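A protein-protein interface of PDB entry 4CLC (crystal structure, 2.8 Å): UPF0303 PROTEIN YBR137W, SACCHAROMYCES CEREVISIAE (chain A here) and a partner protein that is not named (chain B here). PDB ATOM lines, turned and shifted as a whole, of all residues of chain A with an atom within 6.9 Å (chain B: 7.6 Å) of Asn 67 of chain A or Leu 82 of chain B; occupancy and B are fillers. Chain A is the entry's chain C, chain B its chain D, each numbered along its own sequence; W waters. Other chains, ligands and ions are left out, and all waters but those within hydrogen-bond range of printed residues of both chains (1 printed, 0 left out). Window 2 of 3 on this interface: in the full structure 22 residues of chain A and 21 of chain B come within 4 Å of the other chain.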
ATOM      1  N   SER A  64     -17.604 -10.430  14.024  1.00  0.00           N
ATOM      2  CA  SER A  64     -18.627 -11.460  13.881  1.00  0.00           C
ATOM      3  C   SER A  64     -18.220 -12.478  12.853  1.00  0.00           C
ATOM      4  O   SER A  64     -17.464 -12.165  11.961  1.00  0.00           O
ATOM      5  CB  SER A  64     -19.963 -10.858  13.464  1.00  0.00           C
ATOM      6  OG  SER A  64     -20.513 -10.058  14.488  1.00  0.00           O
ATOM      7  N   LEU A  65     -18.739 -13.692  12.963  1.00  0.00           N
ATOM      8  CA  LEU A  65     -18.515 -14.708  11.947  1.00  0.00           C
ATOM      9  C   LEU A  65     -19.419 -14.446  10.747  1.00  0.00           C
ATOM     10  O   LEU A  65     -20.383 -13.693  10.842  1.00  0.00           O
ATOM     11  CB  LEU A  65     -18.776 -16.112  12.504  1.00  0.00           C
ATOM     12  CG  LEU A  65     -18.128 -16.577  13.806  1.00  0.00           C
ATOM     13  CD1 LEU A  65     -18.453 -18.037  13.982  1.00  0.00           C
ATOM     14  CD2 LEU A  65     -16.633 -16.345  13.815  1.00  0.00           C
ATOM     15  N   PRO A  66     -19.110 -15.075   9.612  1.00  0.00           N
ATOM     16  CA  PRO A  66     -19.963 -14.945   8.433  1.00  0.00           C
ATOM     17  C   PRO A  66     -21.377 -15.446   8.627  1.00  0.00           C
ATOM     18  O   PRO A  66     -22.221 -15.112   7.805  1.00  0.00           O
ATOM     19  CB  PRO A  66     -19.245 -15.797   7.392  1.00  0.00           C
ATOM     20  CG  PRO A  66     -17.817 -15.777   7.818  1.00  0.00           C
ATOM     21  CD  PRO A  66     -17.868 -15.809   9.310  1.00  0.00           C
ATOM     22  N   ASN A  67     -21.651 -16.240   9.657  1.00  0.00           N
ATOM     23  CA  ASN A  67     -23.032 -16.660   9.902  1.00  0.00           C
ATOM     24  C   ASN A  67     -23.756 -15.712  10.867  1.00  0.00           C
ATOM     25  O   ASN A  67     -24.958 -15.860  11.126  1.00  0.00           O
ATOM     26  CB  ASN A  67     -23.070 -18.090  10.434  1.00  0.00           C
ATOM     27  CG  ASN A  67     -22.597 -18.198  11.872  1.00  0.00           C
ATOM     28  OD1 ASN A  67     -21.852 -17.354  12.380  1.00  0.00           O
ATOM     29  ND2 ASN A  67     -23.031 -19.252  12.536  1.00  0.00           N
ATOM     30  N   GLY A  68     -23.006 -14.747  11.400  1.00  0.00           N
ATOM     31  CA  GLY A  68     -23.550 -13.717  12.262  1.00  0.00           C
ATOM     32  C   GLY A  68     -23.218 -13.814  13.733  1.00  0.00           C
ATOM     33  O   GLY A  68     -23.452 -12.869  14.472  1.00  0.00           O
ATOM     34  N   HIS A  69     -22.687 -14.948  14.175  1.00  0.00           N
ATOM     35  CA  HIS A  69     -22.354 -15.094  15.589  1.00  0.00           C
ATOM     36  C   HIS A  69     -21.397 -13.989  16.013  1.00  0.00           C
ATOM     37  O   HIS A  69     -20.293 -13.906  15.523  1.00  0.00           O
ATOM     38  CB  HIS A  69     -21.735 -16.474  15.849  1.00  0.00           C
ATOM     39  CG  HIS A  69     -21.265 -16.680  17.260  1.00  0.00           C
ATOM     40  ND1 HIS A  69     -21.826 -16.030  18.341  1.00  0.00           N
ATOM     41  CD2 HIS A  69     -20.289 -17.474  17.766  1.00  0.00           C
ATOM     42  CE1 HIS A  69     -21.208 -16.397  19.444  1.00  0.00           C
ATOM     43  NE2 HIS A  69     -20.274 -17.279  19.131  1.00  0.00           N
ATOM     44  N   CYS A  70     -21.809 -13.173  16.969  1.00  0.00           N
ATOM     45  CA  CYS A  70     -21.008 -12.045  17.382  1.00  0.00           C
ATOM     46  C   CYS A  70     -20.065 -12.447  18.500  1.00  0.00           C
ATOM     47  O   CYS A  70     -20.500 -12.958  19.534  1.00  0.00           O
ATOM     48  CB  CYS A  70     -21.900 -10.891  17.815  1.00  0.00           C
ATOM     49  SG  CYS A  70     -21.005  -9.505  18.538  1.00  0.00           S
ATOM     50  N   LYS A  92     -21.559  -4.631   7.453  1.00  0.00           N
ATOM     51  CA  LYS A  92     -21.121  -6.015   7.611  1.00  0.00           C
ATOM     52  C   LYS A  92     -21.796  -6.915   6.589  1.00  0.00           C
ATOM     53  O   LYS A  92     -21.175  -7.817   6.024  1.00  0.00           O
ATOM     54  CB  LYS A  92     -21.405  -6.492   9.037  1.00  0.00           C
ATOM     55  CG  LYS A  92     -20.929  -7.876   9.381  1.00  0.00           C
ATOM     56  CD  LYS A  92     -21.037  -8.149  10.904  1.00  0.00           C
ATOM     57  CE  LYS A  92     -22.491  -8.150  11.421  1.00  0.00           C
ATOM     58  NZ  LYS A  92     -23.312  -9.224  10.778  1.00  0.00           N
ATOM     59  N   LEU A  96     -19.728  -9.120   3.817  1.00  0.00           N
ATOM     60  CA  LEU A  96     -19.829 -10.570   3.857  1.00  0.00           C
ATOM     61  C   LEU A  96     -20.416 -11.080   2.563  1.00  0.00           C
ATOM     62  O   LEU A  96     -19.990 -12.111   2.049  1.00  0.00           O
ATOM     63  CB  LEU A  96     -20.659 -11.038   5.067  1.00  0.00           C
ATOM     64  CG  LEU A  96     -19.902 -11.159   6.399  1.00  0.00           C
ATOM     65  CD1 LEU A  96     -20.822 -11.370   7.565  1.00  0.00           C
ATOM     66  CD2 LEU A  96     -18.911 -12.286   6.313  1.00  0.00           C
ATOM     67  N   GLY B  79     -16.096 -22.874  21.102  1.00  0.00           N
ATOM     68  CA  GLY B  79     -17.329 -23.631  21.084  1.00  0.00           C
ATOM     69  C   GLY B  79     -18.596 -22.862  21.415  1.00  0.00           C
ATOM     70  O   GLY B  79     -19.634 -23.479  21.649  1.00  0.00           O
ATOM     71  N   SER B  80     -18.527 -21.530  21.443  1.00  0.00           N
ATOM     72  CA  SER B  80     -19.746 -20.735  21.455  1.00  0.00           C
ATOM     73  C   SER B  80     -20.314 -20.773  20.052  1.00  0.00           C
ATOM     74  O   SER B  80     -19.668 -21.276  19.125  1.00  0.00           O
ATOM     75  CB  SER B  80     -19.486 -19.299  21.871  1.00  0.00           C
ATOM     76  OG  SER B  80     -18.783 -18.596  20.853  1.00  0.00           O
ATOM     77  N   ALA B  81     -21.515 -20.230  19.886  1.00  0.00           N
ATOM     78  CA  ALA B  81     -22.214 -20.364  18.612  1.00  0.00           C
ATOM     79  C   ALA B  81     -23.305 -19.331  18.476  1.00  0.00           C
ATOM     80  O   ALA B  81     -23.713 -18.723  19.452  1.00  0.00           O
ATOM     81  CB  ALA B  81     -22.796 -21.756  18.458  1.00  0.00           C
ATOM     82  N   LEU B  82     -23.806 -19.180  17.258  1.00  0.00           N
ATOM     83  CA  LEU B  82     -25.088 -18.543  17.042  1.00  0.00           C
ATOM     84  C   LEU B  82     -26.068 -19.380  17.863  1.00  0.00           C
ATOM     85  O   LEU B  82     -25.777 -20.531  18.204  1.00  0.00           O
ATOM     86  CB  LEU B  82     -25.443 -18.555  15.553  1.00  0.00           C
ATOM     87  CG  LEU B  82     -26.545 -17.702  14.922  1.00  0.00           C
ATOM     88  CD1 LEU B  82     -26.277 -16.206  15.074  1.00  0.00           C
ATOM     89  CD2 LEU B  82     -26.635 -18.086  13.476  1.00  0.00           C
ATOM     90  N   ASP B  83     -27.208 -18.806  18.202  1.00  0.00           N
ATOM     91  CA  ASP B  83     -28.143 -19.372  19.201  1.00  0.00           C
ATOM     92  C   ASP B  83     -27.675 -19.005  20.609  1.00  0.00           C
ATOM     93  O   ASP B  83     -28.515 -18.769  21.479  1.00  0.00           O
ATOM     94  CB  ASP B  83     -28.296 -20.911  19.036  1.00  0.00           C
ATOM     95  CG  ASP B  83     -28.996 -21.571  20.194  1.00  0.00           C
ATOM     96  OD1 ASP B  83     -30.247 -21.605  20.201  1.00  0.00           O
ATOM     97  OD2 ASP B  83     -28.287 -22.085  21.090  1.00  0.00           O
ATOM     98  N   ASN B  84     -26.385 -18.738  20.794  1.00  0.00           N
ATOM     99  CA  ASN B  84     -26.022 -17.964  21.962  1.00  0.00           C
ATOM    100  C   ASN B  84     -26.578 -16.568  21.788  1.00  0.00           C
ATOM    101  O   ASN B  84     -26.994 -15.925  22.742  1.00  0.00           O
ATOM    102  CB  ASN B  84     -24.520 -17.909  22.175  1.00  0.00           C
ATOM    103  CG  ASN B  84     -23.983 -19.154  22.824  1.00  0.00           C
ATOM    104  OD1 ASN B  84     -23.177 -19.869  22.234  1.00  0.00           O
ATOM    105  ND2 ASN B  84     -24.421 -19.424  24.050  1.00  0.00           N
ATOM    106  N   ASP B  85     -26.601 -16.111  20.542  1.00  0.00           N
ATOM    107  CA  ASP B  85     -27.104 -14.780  20.229  1.00  0.00           C
ATOM    108  C   ASP B  85     -28.626 -14.745  20.327  1.00  0.00           C
ATOM    109  O   ASP B  85     -29.201 -13.814  20.905  1.00  0.00           O
ATOM    110  CB  ASP B  85     -26.638 -14.339  18.841  1.00  0.00           C
ATOM    111  CG  ASP B  85     -25.145 -14.099  18.773  1.00  0.00           C
ATOM    112  OD1 ASP B  85     -24.515 -13.764  19.804  1.00  0.00           O
ATOM    113  OD2 ASP B  85     -24.581 -14.260  17.685  1.00  0.00           O
ATOM    114  N   PHE B  86     -29.271 -15.761  19.767  1.00  0.00           N
ATOM    115  CA  PHE B  86     -30.706 -15.906  19.911  1.00  0.00           C
ATOM    116  C   PHE B  86     -31.112 -15.925  21.393  1.00  0.00           C
ATOM    117  O   PHE B  86     -32.019 -15.196  21.802  1.00  0.00           O
ATOM    118  CB  PHE B  86     -31.175 -17.173  19.211  1.00  0.00           C
ATOM    119  CG  PHE B  86     -31.201 -17.063  17.724  1.00  0.00           C
ATOM    120  CD1 PHE B  86     -32.313 -16.528  17.076  1.00  0.00           C
ATOM    121  CD2 PHE B  86     -30.118 -17.491  16.959  1.00  0.00           C
ATOM    122  CE1 PHE B  86     -32.356 -16.411  15.699  1.00  0.00           C
ATOM    123  CE2 PHE B  86     -30.148 -17.387  15.571  1.00  0.00           C
ATOM    124  CZ  PHE B  86     -31.284 -16.839  14.945  1.00  0.00           C
ATOM    125  N   TRP B  87     -30.418 -16.741  22.192  1.00  0.00           N
ATOM    126  CA  TRP B  87     -30.739 -16.856  23.611  1.00  0.00           C
ATOM    127  C   TRP B  87     -30.545 -15.522  24.286  1.00  0.00           C
ATOM    128  O   TRP B  87     -31.385 -15.097  25.085  1.00  0.00           O
ATOM    129  CB  TRP B  87     -29.896 -17.943  24.307  1.00  0.00           C
ATOM    130  CG  TRP B  87     -30.536 -19.302  24.198  1.00  0.00           C
ATOM    131  CD1 TRP B  87     -30.239 -20.288  23.297  1.00  0.00           C
ATOM    132  CD2 TRP B  87     -31.612 -19.795  24.984  1.00  0.00           C
ATOM    133  NE1 TRP B  87     -31.067 -21.361  23.473  1.00  0.00           N
ATOM    134  CE2 TRP B  87     -31.924 -21.085  24.515  1.00  0.00           C
ATOM    135  CE3 TRP B  87     -32.350 -19.274  26.049  1.00  0.00           C
ATOM    136  CZ2 TRP B  87     -32.932 -21.866  25.075  1.00  0.00           C
ATOM    137  CZ3 TRP B  87     -33.354 -20.046  26.603  1.00  0.00           C
ATOM    138  CH2 TRP B  87     -33.636 -21.325  26.117  1.00  0.00           C
HETATM  139  O   HOH W   1     -22.925 -20.493  14.916  1.00  0.00           O
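Leu 82 of chain B touches Asn 67 of chain A (CD2 to O, 3.6 Å). Gly 68 of chain A touches Asp 85 of chain B (O to OD2, 3.7 Å). CG of His 69 of chain A touches N of Leu 82 of chain B (3.6 Å).
ND1 of His 69 of chain A sits close to OD2 of Asp 85 of chain B, 3.3 Å away. The backbone NH (N) of Cys 70 of chain A sits at hydrogen-bond distance from the side-chain carboxylate (OD2) of Asp 85 of chain B (3.1 Å). A ring nitrogen (NE2) of His 69 of chain A sits at hydrogen-bond distance from the backbone NH (N) of Ala 81 of chain B (3.3 Å). NE2 of His 69 of chain A lies within hydrogen-bond range of OG of Ser 80 of chain B.
Water W1 lies within hydrogen-bond range of ND2 of Asn 67 of chain A and N of Leu 82 of chain B.
The backbone NH (N) of Ala 81 of chain B lies within hydrogen-bond range of the side-chain amide oxygen (OD1) of Asn 84 of chain B. The backbone NH (N) of His 69 of chain A sits at hydrogen-bond distance from the side-chain amide oxygen (OD1) of Asn 67 of chain A (3.1 Å).
Printed residues of chain A within 4 Å of Ser 80 of chain B: His 69. Of the printed residues of chain A, Ala 81 of chain B touches His 69. Of chain A, only Asn 67 (3.6 Å) and His 69 (3.6 Å) come within 4 Å of Leu 82 of chain B. The nearest residue of chain B that does not touch Asn 67 of chain A is Ala 81 of chain B (5.9 Å). The nearest residue of chain A that does not touch Leu 82 of chain B is Gly 68 of chain A (4.1 Å).
Of the 9 printed residues of chain A, 4 touch a printed residue of chain B. Hydrophobic or aromatic side chains of chain A within 4 Å of the printed part of chain B: His 69. Hydrophobic or aromatic side chains of chain B within 4 Å of the printed part of chain A: Leu 82. Among the printed residues, 7 pairs touch across the chains. Among the printed residues, no Asp or Glu carboxylate lies within 4 Å of a Lys or Arg side-chain nitrogen of the other chain.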
